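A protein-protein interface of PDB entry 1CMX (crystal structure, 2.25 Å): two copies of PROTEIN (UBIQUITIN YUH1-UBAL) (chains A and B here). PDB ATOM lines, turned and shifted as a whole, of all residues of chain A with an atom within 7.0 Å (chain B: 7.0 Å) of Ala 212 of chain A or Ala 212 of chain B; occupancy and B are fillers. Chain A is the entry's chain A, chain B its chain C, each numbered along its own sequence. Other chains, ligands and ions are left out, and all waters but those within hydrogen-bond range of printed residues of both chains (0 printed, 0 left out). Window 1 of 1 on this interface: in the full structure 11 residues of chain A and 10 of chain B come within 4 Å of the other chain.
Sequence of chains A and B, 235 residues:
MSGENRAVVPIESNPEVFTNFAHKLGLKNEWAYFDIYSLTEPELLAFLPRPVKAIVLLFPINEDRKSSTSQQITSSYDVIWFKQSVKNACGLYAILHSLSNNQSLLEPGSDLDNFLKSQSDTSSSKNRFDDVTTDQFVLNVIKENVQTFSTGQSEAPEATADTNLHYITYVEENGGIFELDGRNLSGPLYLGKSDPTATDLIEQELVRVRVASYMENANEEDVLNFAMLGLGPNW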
ATOM      1  N   LEU A  39      15.766   0.758 -15.032  1.00  0.00           N
ATOM      2  CA  LEU A  39      14.458   0.151 -15.214  1.00  0.00           C
ATOM      3  C   LEU A  39      13.756  -0.259 -13.909  1.00  0.00           C
ATOM      4  O   LEU A  39      13.535  -1.454 -13.620  1.00  0.00           O
ATOM      5  CB  LEU A  39      14.571  -1.013 -16.197  1.00  0.00           C
ATOM      6  CG  LEU A  39      13.266  -1.673 -16.618  1.00  0.00           C
ATOM      7  CD1 LEU A  39      12.345  -0.693 -17.337  1.00  0.00           C
ATOM      8  CD2 LEU A  39      13.605  -2.841 -17.496  1.00  0.00           C
ATOM      9  N   THR A  40      13.387   0.814 -13.212  1.00  0.00           N
ATOM     10  CA  THR A  40      12.666   0.931 -11.947  1.00  0.00           C
ATOM     11  C   THR A  40      13.287   2.148 -11.261  1.00  0.00           C
ATOM     12  O   THR A  40      13.750   2.117 -10.110  1.00  0.00           O
ATOM     13  CB  THR A  40      12.686  -0.305 -11.014  1.00  0.00           C
ATOM     14  OG1 THR A  40      11.973  -1.394 -11.630  1.00  0.00           O
ATOM     15  CG2 THR A  40      11.942   0.064  -9.751  1.00  0.00           C
ATOM     16  N   VAL A 207       7.075  -7.206 -18.036  1.00  0.00           N
ATOM     17  CA  VAL A 207       8.336  -6.971 -18.728  1.00  0.00           C
ATOM     18  C   VAL A 207       9.452  -6.765 -17.687  1.00  0.00           C
ATOM     19  O   VAL A 207      10.486  -7.447 -17.738  1.00  0.00           O
ATOM     20  CB  VAL A 207       8.263  -5.738 -19.672  1.00  0.00           C
ATOM     21  CG1 VAL A 207       9.644  -5.493 -20.342  1.00  0.00           C
ATOM     22  CG2 VAL A 207       7.207  -5.952 -20.715  1.00  0.00           C
ATOM     23  N   ARG A 208       9.226  -5.841 -16.754  1.00  0.00           N
ATOM     24  CA  ARG A 208      10.189  -5.553 -15.684  1.00  0.00           C
ATOM     25  C   ARG A 208      10.582  -6.826 -14.952  1.00  0.00           C
ATOM     26  O   ARG A 208      11.769  -7.096 -14.714  1.00  0.00           O
ATOM     27  CB  ARG A 208       9.605  -4.565 -14.676  1.00  0.00           C
ATOM     28  CG  ARG A 208       9.618  -3.143 -15.098  1.00  0.00           C
ATOM     29  CD  ARG A 208       8.655  -2.326 -14.258  1.00  0.00           C
ATOM     30  NE  ARG A 208       8.868  -0.881 -14.398  1.00  0.00           N
ATOM     31  CZ  ARG A 208       7.991   0.053 -14.011  1.00  0.00           C
ATOM     32  NH1 ARG A 208       6.833  -0.308 -13.457  1.00  0.00           N
ATOM     33  NH2 ARG A 208       8.273   1.354 -14.159  1.00  0.00           N
ATOM     34  N   VAL A 209       9.604  -7.675 -14.696  1.00  0.00           N
ATOM     35  CA  VAL A 209       9.929  -8.891 -13.989  1.00  0.00           C
ATOM     36  C   VAL A 209      10.702  -9.877 -14.838  1.00  0.00           C
ATOM     37  O   VAL A 209      11.596 -10.569 -14.351  1.00  0.00           O
ATOM     38  CB  VAL A 209       8.672  -9.523 -13.367  1.00  0.00           C
ATOM     39  CG1 VAL A 209       8.999 -10.874 -12.835  1.00  0.00           C
ATOM     40  CG2 VAL A 209       8.117  -8.587 -12.253  1.00  0.00           C
ATOM     41  N   ARG A 210      10.316 -10.006 -16.099  1.00  0.00           N
ATOM     42  CA  ARG A 210      11.008 -10.915 -16.996  1.00  0.00           C
ATOM     43  C   ARG A 210      12.488 -10.404 -17.162  1.00  0.00           C
ATOM     44  O   ARG A 210      13.442 -11.154 -17.145  1.00  0.00           O
ATOM     45  CB  ARG A 210      10.259 -10.849 -18.341  1.00  0.00           C
ATOM     46  CG  ARG A 210      10.783 -11.715 -19.466  1.00  0.00           C
ATOM     47  CD  ARG A 210      10.691 -13.125 -19.093  1.00  0.00           C
ATOM     48  NE  ARG A 210      11.152 -13.999 -20.143  1.00  0.00           N
ATOM     49  CZ  ARG A 210      10.983 -15.312 -20.125  1.00  0.00           C
ATOM     50  NH1 ARG A 210      10.349 -15.875 -19.098  1.00  0.00           N
ATOM     51  NH2 ARG A 210      11.457 -16.059 -21.123  1.00  0.00           N
ATOM     52  N   VAL A 211      12.649  -9.107 -17.286  1.00  0.00           N
ATOM     53  CA  VAL A 211      13.968  -8.549 -17.493  1.00  0.00           C
ATOM     54  C   VAL A 211      14.794  -8.705 -16.222  1.00  0.00           C
ATOM     55  O   VAL A 211      15.934  -9.232 -16.260  1.00  0.00           O
ATOM     56  CB  VAL A 211      13.875  -7.077 -17.896  1.00  0.00           C
ATOM     57  CG1 VAL A 211      15.275  -6.398 -17.732  1.00  0.00           C
ATOM     58  CG2 VAL A 211      13.394  -6.955 -19.342  1.00  0.00           C
ATOM     59  N   ALA A 212      14.179  -8.326 -15.096  1.00  0.00           N
ATOM     60  CA  ALA A 212      14.869  -8.402 -13.834  1.00  0.00           C
ATOM     61  C   ALA A 212      15.333  -9.796 -13.538  1.00  0.00           C
ATOM     62  O   ALA A 212      16.414  -9.975 -12.978  1.00  0.00           O
ATOM     63  CB  ALA A 212      14.058  -7.800 -12.703  1.00  0.00           C
ATOM     64  N   SER A 213      14.649 -10.778 -14.108  1.00  0.00           N
ATOM     65  CA  SER A 213      15.061 -12.151 -13.876  1.00  0.00           C
ATOM     66  C   SER A 213      16.366 -12.486 -14.588  1.00  0.00           C
ATOM     67  O   SER A 213      17.068 -13.420 -14.181  1.00  0.00           O
ATOM     68  CB  SER A 213      13.953 -13.102 -14.313  1.00  0.00           C
ATOM     69  OG  SER A 213      14.444 -14.404 -14.602  1.00  0.00           O
ATOM     70  N   TYR A 214      16.619 -11.828 -15.725  1.00  0.00           N
ATOM     71  CA  TYR A 214      17.867 -12.058 -16.463  1.00  0.00           C
ATOM     72  C   TYR A 214      19.030 -11.402 -15.685  1.00  0.00           C
ATOM     73  O   TYR A 214      20.043 -12.029 -15.428  1.00  0.00           O
ATOM     74  CB  TYR A 214      17.760 -11.490 -17.886  1.00  0.00           C
ATOM     75  CG  TYR A 214      16.809 -12.263 -18.755  1.00  0.00           C
ATOM     76  CD1 TYR A 214      15.786 -11.626 -19.420  1.00  0.00           C
ATOM     77  CD2 TYR A 214      16.998 -13.612 -18.984  1.00  0.00           C
ATOM     78  CE1 TYR A 214      14.988 -12.307 -20.314  1.00  0.00           C
ATOM     79  CE2 TYR A 214      16.194 -14.312 -19.888  1.00  0.00           C
ATOM     80  CZ  TYR A 214      15.197 -13.648 -20.556  1.00  0.00           C
ATOM     81  OH  TYR A 214      14.419 -14.311 -21.511  1.00  0.00           O
ATOM     82  N   MET A 215      18.823 -10.171 -15.232  1.00  0.00           N
ATOM     83  CA  MET A 215      19.832  -9.457 -14.485  1.00  0.00           C
ATOM     84  C   MET A 215      20.283 -10.209 -13.239  1.00  0.00           C
ATOM     85  O   MET A 215      21.451 -10.134 -12.880  1.00  0.00           O
ATOM     86  CB  MET A 215      19.314  -8.094 -14.064  1.00  0.00           C
ATOM     87  CG  MET A 215      18.441  -7.508 -15.064  1.00  0.00           C
ATOM     88  SD  MET A 215      18.507  -5.774 -15.068  1.00  0.00           S
ATOM     89  CE  MET A 215      17.252  -5.234 -14.082  1.00  0.00           C
ATOM     90  N   GLU A 216      19.357 -10.927 -12.599  1.00  0.00           N
ATOM     91  CA  GLU A 216      19.663 -11.673 -11.385  1.00  0.00           C
ATOM     92  C   GLU A 216      20.704 -12.735 -11.672  1.00  0.00           C
ATOM     93  O   GLU A 216      21.589 -12.988 -10.840  1.00  0.00           O
ATOM     94  CB  GLU A 216      18.389 -12.292 -10.770  1.00  0.00           C
ATOM     95  CG  GLU A 216      18.636 -13.211  -9.581  1.00  0.00           C
ATOM     96  CD  GLU A 216      19.433 -12.531  -8.479  1.00  0.00           C
ATOM     97  OE1 GLU A 216      20.297 -13.208  -7.909  1.00  0.00           O
ATOM     98  OE2 GLU A 216      19.262 -11.314  -8.216  1.00  0.00           O
ATOM     99  N   ASN A 217      20.618 -13.356 -12.845  1.00  0.00           N
ATOM    100  CA  ASN A 217      21.602 -14.373 -13.213  1.00  0.00           C
ATOM    101  C   ASN A 217      22.989 -13.693 -13.448  1.00  0.00           C
ATOM    102  O   ASN A 217      24.037 -14.190 -13.004  1.00  0.00           O
ATOM    103  CB  ASN A 217      21.115 -15.156 -14.426  1.00  0.00           C
ATOM    104  CG  ASN A 217      21.652 -16.573 -14.445  1.00  0.00           C
ATOM    105  OD1 ASN A 217      22.397 -16.960 -15.347  1.00  0.00           O
ATOM    106  ND2 ASN A 217      21.284 -17.356 -13.434  1.00  0.00           N
ATOM    107  N   ASN A 219      24.033 -10.682 -11.979  1.00  0.00           N
ATOM    108  CA  ASN A 219      24.507 -10.309 -10.657  1.00  0.00           C
ATOM    109  C   ASN A 219      25.209 -11.457  -9.936  1.00  0.00           C
ATOM    110  O   ASN A 219      26.219 -11.239  -9.263  1.00  0.00           O
ATOM    111  CB  ASN A 219      23.356  -9.734  -9.840  1.00  0.00           C
ATOM    112  CG  ASN A 219      22.953  -8.361 -10.324  1.00  0.00           C
ATOM    113  OD1 ASN A 219      23.625  -7.767 -11.153  1.00  0.00           O
ATOM    114  ND2 ASN A 219      21.841  -7.868  -9.841  1.00  0.00           N
ATOM    115  N   PHE A 226      24.999  -5.940 -20.008  1.00  0.00           N
ATOM    116  CA  PHE A 226      23.578  -5.794 -20.220  1.00  0.00           C
ATOM    117  C   PHE A 226      23.357  -4.425 -20.704  1.00  0.00           C
ATOM    118  O   PHE A 226      23.942  -3.472 -20.184  1.00  0.00           O
ATOM    119  CB  PHE A 226      22.758  -5.860 -18.903  1.00  0.00           C
ATOM    120  CG  PHE A 226      22.240  -7.219 -18.548  1.00  0.00           C
ATOM    121  CD1 PHE A 226      23.110  -8.232 -18.224  1.00  0.00           C
ATOM    122  CD2 PHE A 226      20.879  -7.475 -18.507  1.00  0.00           C
ATOM    123  CE1 PHE A 226      22.633  -9.488 -17.861  1.00  0.00           C
ATOM    124  CE2 PHE A 226      20.397  -8.731 -18.149  1.00  0.00           C
ATOM    125  CZ  PHE A 226      21.271  -9.730 -17.831  1.00  0.00           C
ATOM    126  N   LEU B  39       5.855  -3.386  -6.161  1.00  0.00           N
ATOM    127  CA  LEU B  39       7.270  -3.101  -6.226  1.00  0.00           C
ATOM    128  C   LEU B  39       7.963  -2.677  -7.481  1.00  0.00           C
ATOM    129  O   LEU B  39       8.614  -3.504  -8.116  1.00  0.00           O
ATOM    130  CB  LEU B  39       8.138  -4.205  -5.668  1.00  0.00           C
ATOM    131  CG  LEU B  39       8.364  -4.382  -4.181  1.00  0.00           C
ATOM    132  CD1 LEU B  39       9.404  -5.459  -4.070  1.00  0.00           C
ATOM    133  CD2 LEU B  39       8.843  -3.126  -3.488  1.00  0.00           C
ATOM    134  N   GLU B 205      17.865  -1.579  -6.034  1.00  0.00           N
ATOM    135  CA  GLU B 205      17.791  -2.378  -7.239  1.00  0.00           C
ATOM    136  C   GLU B 205      18.190  -3.813  -6.951  1.00  0.00           C
ATOM    137  O   GLU B 205      17.585  -4.746  -7.473  1.00  0.00           O
ATOM    138  CB  GLU B 205      18.765  -1.781  -8.264  1.00  0.00           C
ATOM    139  CG  GLU B 205      18.142  -0.841  -9.243  1.00  0.00           C
ATOM    140  CD  GLU B 205      17.444  -1.621 -10.345  1.00  0.00           C
ATOM    141  OE1 GLU B 205      18.141  -2.451 -11.001  1.00  0.00           O
ATOM    142  OE2 GLU B 205      16.210  -1.429 -10.523  1.00  0.00           O
ATOM    143  N   VAL B 207      17.640  -5.603  -4.440  1.00  0.00           N
ATOM    144  CA  VAL B 207      16.553  -6.353  -3.776  1.00  0.00           C
ATOM    145  C   VAL B 207      15.453  -6.623  -4.795  1.00  0.00           C
ATOM    146  O   VAL B 207      14.970  -7.740  -4.915  1.00  0.00           O
ATOM    147  CB  VAL B 207      15.945  -5.602  -2.504  1.00  0.00           C
ATOM    148  CG1 VAL B 207      14.714  -6.390  -1.955  1.00  0.00           C
ATOM    149  CG2 VAL B 207      16.959  -5.569  -1.425  1.00  0.00           C
ATOM    150  N   ARG B 208      15.016  -5.574  -5.482  1.00  0.00           N
ATOM    151  CA  ARG B 208      13.973  -5.683  -6.515  1.00  0.00           C
ATOM    152  C   ARG B 208      14.307  -6.740  -7.556  1.00  0.00           C
ATOM    153  O   ARG B 208      13.509  -7.619  -7.868  1.00  0.00           O
ATOM    154  CB  ARG B 208      13.854  -4.365  -7.200  1.00  0.00           C
ATOM    155  CG  ARG B 208      13.415  -3.277  -6.303  1.00  0.00           C
ATOM    156  CD  ARG B 208      13.224  -2.080  -7.163  1.00  0.00           C
ATOM    157  NE  ARG B 208      12.204  -1.164  -6.681  1.00  0.00           N
ATOM    158  CZ  ARG B 208      12.316   0.160  -6.785  1.00  0.00           C
ATOM    159  NH1 ARG B 208      13.414   0.683  -7.348  1.00  0.00           N
ATOM    160  NH2 ARG B 208      11.327   0.961  -6.380  1.00  0.00           N
ATOM    161  N   VAL B 209      15.559  -6.743  -7.985  1.00  0.00           N
ATOM    162  CA  VAL B 209      16.013  -7.710  -8.978  1.00  0.00           C
ATOM    163  C   VAL B 209      15.979  -9.127  -8.403  1.00  0.00           C
ATOM    164  O   VAL B 209      15.556 -10.074  -9.070  1.00  0.00           O
ATOM    165  CB  VAL B 209      17.487  -7.322  -9.488  1.00  0.00           C
ATOM    166  CG1 VAL B 209      18.258  -8.512  -9.984  1.00  0.00           C
ATOM    167  CG2 VAL B 209      17.427  -6.210 -10.515  1.00  0.00           C
ATOM    168  N   ARG B 210      16.529  -9.303  -7.210  1.00  0.00           N
ATOM    169  CA  ARG B 210      16.544 -10.633  -6.617  1.00  0.00           C
ATOM    170  C   ARG B 210      15.087 -11.114  -6.339  1.00  0.00           C
ATOM    171  O   ARG B 210      14.746 -12.274  -6.590  1.00  0.00           O
ATOM    172  CB  ARG B 210      17.390 -10.651  -5.344  1.00  0.00           C
ATOM    173  CG  ARG B 210      17.314 -11.958  -4.620  1.00  0.00           C
ATOM    174  CD  ARG B 210      18.328 -12.926  -5.162  1.00  0.00           C
ATOM    175  NE  ARG B 210      18.458 -14.122  -4.323  1.00  0.00           N
ATOM    176  CZ  ARG B 210      19.403 -15.038  -4.517  1.00  0.00           C
ATOM    177  NH1 ARG B 210      20.257 -14.916  -5.536  1.00  0.00           N
ATOM    178  NH2 ARG B 210      19.664 -15.925  -3.574  1.00  0.00           N
ATOM    179  N   VAL B 211      14.213 -10.207  -5.926  1.00  0.00           N
ATOM    180  CA  VAL B 211      12.812 -10.598  -5.692  1.00  0.00           C
ATOM    181  C   VAL B 211      12.169 -10.947  -7.029  1.00  0.00           C
ATOM    182  O   VAL B 211      11.534 -12.005  -7.187  1.00  0.00           O
ATOM    183  CB  VAL B 211      12.001  -9.430  -5.074  1.00  0.00           C
ATOM    184  CG1 VAL B 211      10.511  -9.682  -5.181  1.00  0.00           C
ATOM    185  CG2 VAL B 211      12.388  -9.246  -3.606  1.00  0.00           C
ATOM    186  N   ALA B 212      12.337 -10.032  -7.986  1.00  0.00           N
ATOM    187  CA  ALA B 212      11.777 -10.172  -9.316  1.00  0.00           C
ATOM    188  C   ALA B 212      12.136 -11.510  -9.926  1.00  0.00           C
ATOM    189  O   ALA B 212      11.301 -12.139 -10.574  1.00  0.00           O
ATOM    190  CB  ALA B 212      12.241  -9.049 -10.194  1.00  0.00           C
ATOM    191  N   SER B 213      13.338 -12.005  -9.637  1.00  0.00           N
ATOM    192  CA  SER B 213      13.700 -13.306 -10.190  1.00  0.00           C
ATOM    193  C   SER B 213      12.913 -14.476  -9.610  1.00  0.00           C
ATOM    194  O   SER B 213      12.872 -15.551 -10.218  1.00  0.00           O
ATOM    195  CB  SER B 213      15.204 -13.623 -10.099  1.00  0.00           C
ATOM    196  OG  SER B 213      15.614 -14.069  -8.818  1.00  0.00           O
ATOM    197  N   TYR B 214      12.425 -14.331  -8.377  1.00  0.00           N
ATOM    198  CA  TYR B 214      11.637 -15.396  -7.767  1.00  0.00           C
ATOM    199  C   TYR B 214      10.257 -15.376  -8.451  1.00  0.00           C
ATOM    200  O   TYR B 214       9.747 -16.406  -8.830  1.00  0.00           O
ATOM    201  CB  TYR B 214      11.512 -15.206  -6.233  1.00  0.00           C
ATOM    202  CG  TYR B 214      12.783 -15.523  -5.446  1.00  0.00           C
ATOM    203  CD1 TYR B 214      13.346 -14.590  -4.589  1.00  0.00           C
ATOM    204  CD2 TYR B 214      13.373 -16.781  -5.524  1.00  0.00           C
ATOM    205  CE1 TYR B 214      14.457 -14.899  -3.810  1.00  0.00           C
ATOM    206  CE2 TYR B 214      14.476 -17.103  -4.759  1.00  0.00           C
ATOM    207  CZ  TYR B 214      15.007 -16.153  -3.893  1.00  0.00           C
ATOM    208  OH  TYR B 214      16.042 -16.486  -3.067  1.00  0.00           O
ATOM    209  N   MET B 215       9.672 -14.198  -8.602  1.00  0.00           N
ATOM    210  CA  MET B 215       8.380 -14.048  -9.239  1.00  0.00           C
ATOM    211  C   MET B 215       8.350 -14.622 -10.666  1.00  0.00           C
ATOM    212  O   MET B 215       7.347 -15.196 -11.081  1.00  0.00           O
ATOM    213  CB  MET B 215       8.010 -12.568  -9.306  1.00  0.00           C
ATOM    214  CG  MET B 215       7.968 -11.858  -7.971  1.00  0.00           C
ATOM    215  SD  MET B 215       7.476 -10.132  -8.117  1.00  0.00           S
ATOM    216  CE  MET B 215       6.726  -9.925  -6.556  1.00  0.00           C
ATOM    217  N   GLU B 216       9.452 -14.480 -11.408  1.00  0.00           N
ATOM    218  CA  GLU B 216       9.512 -14.954 -12.790  1.00  0.00           C
ATOM    219  C   GLU B 216       9.391 -16.465 -12.846  1.00  0.00           C
ATOM    220  O   GLU B 216       8.775 -16.992 -13.770  1.00  0.00           O
ATOM    221  CB  GLU B 216      10.760 -14.388 -13.520  1.00  0.00           C
ATOM    222  CG  GLU B 216      10.880 -14.619 -15.040  1.00  0.00           C
ATOM    223  CD  GLU B 216       9.560 -14.518 -15.839  1.00  0.00           C
ATOM    224  OE1 GLU B 216       9.208 -15.532 -16.449  1.00  0.00           O
ATOM    225  OE2 GLU B 216       8.870 -13.476 -15.855  1.00  0.00           O
ATOM    226  N   ASN B 217       9.944 -17.163 -11.857  1.00  0.00           N
ATOM    227  CA  ASN B 217       9.788 -18.620 -11.808  1.00  0.00           C
ATOM    228  C   ASN B 217       8.322 -18.933 -11.453  1.00  0.00           C
ATOM    229  O   ASN B 217       7.815 -20.026 -11.748  1.00  0.00           O
ATOM    230  CB  ASN B 217      10.705 -19.241 -10.762  1.00  0.00           C
ATOM    231  CG  ASN B 217      12.124 -18.748 -10.876  1.00  0.00           C
ATOM    232  OD1 ASN B 217      12.771 -18.457  -9.863  1.00  0.00           O
ATOM    233  ND2 ASN B 217      12.621 -18.637 -12.112  1.00  0.00           N
ATOM    234  N   ALA B 218       7.647 -17.948 -10.858  1.00  0.00           N
ATOM    235  CA  ALA B 218       6.229 -18.053 -10.474  1.00  0.00           C
ATOM    236  C   ALA B 218       5.273 -17.650 -11.616  1.00  0.00           C
ATOM    237  O   ALA B 218       4.112 -18.061 -11.633  1.00  0.00           O
ATOM    238  CB  ALA B 218       5.944 -17.195  -9.241  1.00  0.00           C
ATOM    239  N   ASN B 219       5.743 -16.794 -12.525  1.00  0.00           N
ATOM    240  CA  ASN B 219       4.939 -16.342 -13.671  1.00  0.00           C
ATOM    241  C   ASN B 219       4.857 -17.427 -14.732  1.00  0.00           C
ATOM    242  O   ASN B 219       3.913 -17.479 -15.527  1.00  0.00           O
ATOM    243  CB  ASN B 219       5.522 -15.068 -14.281  1.00  0.00           C
ATOM    244  CG  ASN B 219       4.948 -13.814 -13.664  1.00  0.00           C
ATOM    245  OD1 ASN B 219       3.949 -13.868 -12.949  1.00  0.00           O
ATOM    246  ND2 ASN B 219       5.568 -12.671 -13.944  1.00  0.00           N
ATOM    247  N   PHE B 226       2.444 -15.285  -3.353  1.00  0.00           N
ATOM    248  CA  PHE B 226       3.496 -14.379  -3.042  1.00  0.00           C
ATOM    249  C   PHE B 226       2.973 -13.302  -2.184  1.00  0.00           C
ATOM    250  O   PHE B 226       1.933 -12.729  -2.506  1.00  0.00           O
ATOM    251  CB  PHE B 226       3.972 -13.724  -4.338  1.00  0.00           C
ATOM    252  CG  PHE B 226       5.200 -14.329  -4.879  1.00  0.00           C
ATOM    253  CD1 PHE B 226       5.150 -15.463  -5.693  1.00  0.00           C
ATOM    254  CD2 PHE B 226       6.419 -13.805  -4.525  1.00  0.00           C
ATOM    255  CE1 PHE B 226       6.319 -16.064  -6.135  1.00  0.00           C
ATOM    256  CE2 PHE B 226       7.589 -14.385  -4.953  1.00  0.00           C
ATOM    257  CZ  PHE B 226       7.549 -15.520  -5.760  1.00  0.00           C
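The backbone carbonyl oxygen (O) of Thr 40 of chain A lies close to the guanidinium group (NH1) of Arg 208 of chain B (3.1 Å). The guanidinium group (NH1) of Arg 210 of chain A is in salt-bridge range of the side-chain carboxylate (OE1) of Glu 216 of chain B. The guanidinium group (NH1) of Arg 210 of chain B lies within salt-bridge range of the side-chain carboxylate (OE1) of Glu 216 of chain A, 2.9 Å away.
The side-chain amide oxygen of Asn 217 of chain B sits close to the backbone carbonyl oxygen of Ser 213 of chain B, 2.9 Å away. NH2 of Arg 210 of chain A is in hydrogen-bond range of OH of Tyr 214 of chain A (3.5 Å). The side-chain hydroxyl (OG) of Ser 213 of chain B is in hydrogen-bond range of the backbone carbonyl oxygen (O) of Arg 210 of chain B (3.0 Å).
Glu 205 of chain B touches Thr 40 of chain A. Val 209 of chain A touches Ala 212 of chain B. Glu 216 of chain B touches Val 209 of chain A (N to CG1, 3.9 Å). O of Ala 212 of chain A touches CG1 of Val 209 of chain B (3.8 Å). CB of Ala 212 of chain B touches CB of Ala 212 of chain A, 3.3 Å away. Glu 216 of chain B touches Ser 213 of chain A (CG to CB, 3.5 Å). Met 215 of chain A touches Val 209 of chain B (CE to CG2, 3.7 Å). Glu 216 of chain A touches Val 209 of chain B. Ser 213 of chain B touches Glu 216 of chain A. Asn 219 of chain A touches Val 209 of chain B.
Of chain B, only Val 209 and Ala 212 come within 4 Å of Ala 212 of chain A. Ala 212 of chain B touches just these residues of chain A: Val 209 (3.5 Å) and Ala 212 (3.3 Å). Of the printed residues of chain A, Glu 216 of chain B touches Val 209, Arg 210 and Ser 213. Of the printed residues of chain A, Arg 210 of chain B touches Glu 216 (2.9 Å). Printed residues of chain B within 4 Å of Asn 219 of chain A: Val 209 (3.6 Å). Ala 218 of chain B touches none of the printed residues of chain A. Met 215 of chain B touches none of the printed residues of chain A. The nearest printed residue of chain B that does not touch Asn 219 of chain A is Glu 205 of chain B (5.8 Å).
Hydrophobic or aromatic side chains of chain A that line the printed part of chain B: Val 209, Ala 212 and Met 215. Along chain A the printed residues that touch a printed residue of chain B span positions 40 to 219. Hydrophobic or aromatic side chains of chain B within 4 Å of the printed part of chain A: Val 209 and Ala 212. Along chain B the printed residues that touch a printed residue of chain A span positions 205 to 216. Among the printed residues, 13 pairs touch across the chains. Among the printed residues, Asp or Glu carboxylates within 4 Å of a Lys or Arg side-chain nitrogen of the other chain: Arg 210 of chain A with Glu 216 of chain B and Glu 216 of chain A with Arg 210 of chain B.
Val 209 of chain A touches Ala 212 of chain B, and with the chains exchanged Ala 212 of chain A touches Val 209 of chain B. Ser 213 of chain A touches Glu 216 of chain B, and with the chains exchanged Glu 216 of chain A touches Ser 213 of chain B. Met 215 of chain A touches Val 209 of chain B, but with the chains exchanged Val 209 of chain A does not touch Met 215 of chain B (4.04 Å). Asn 219 of chain A touches Val 209 of chain B, but with the chains exchanged Val 209 of chain A does not touch Asn 219 of chain B (4.03 Å). Of the 13 pairs that touch across the chains among the printed residues, 9 have their exchanged pair printed and touching as well.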
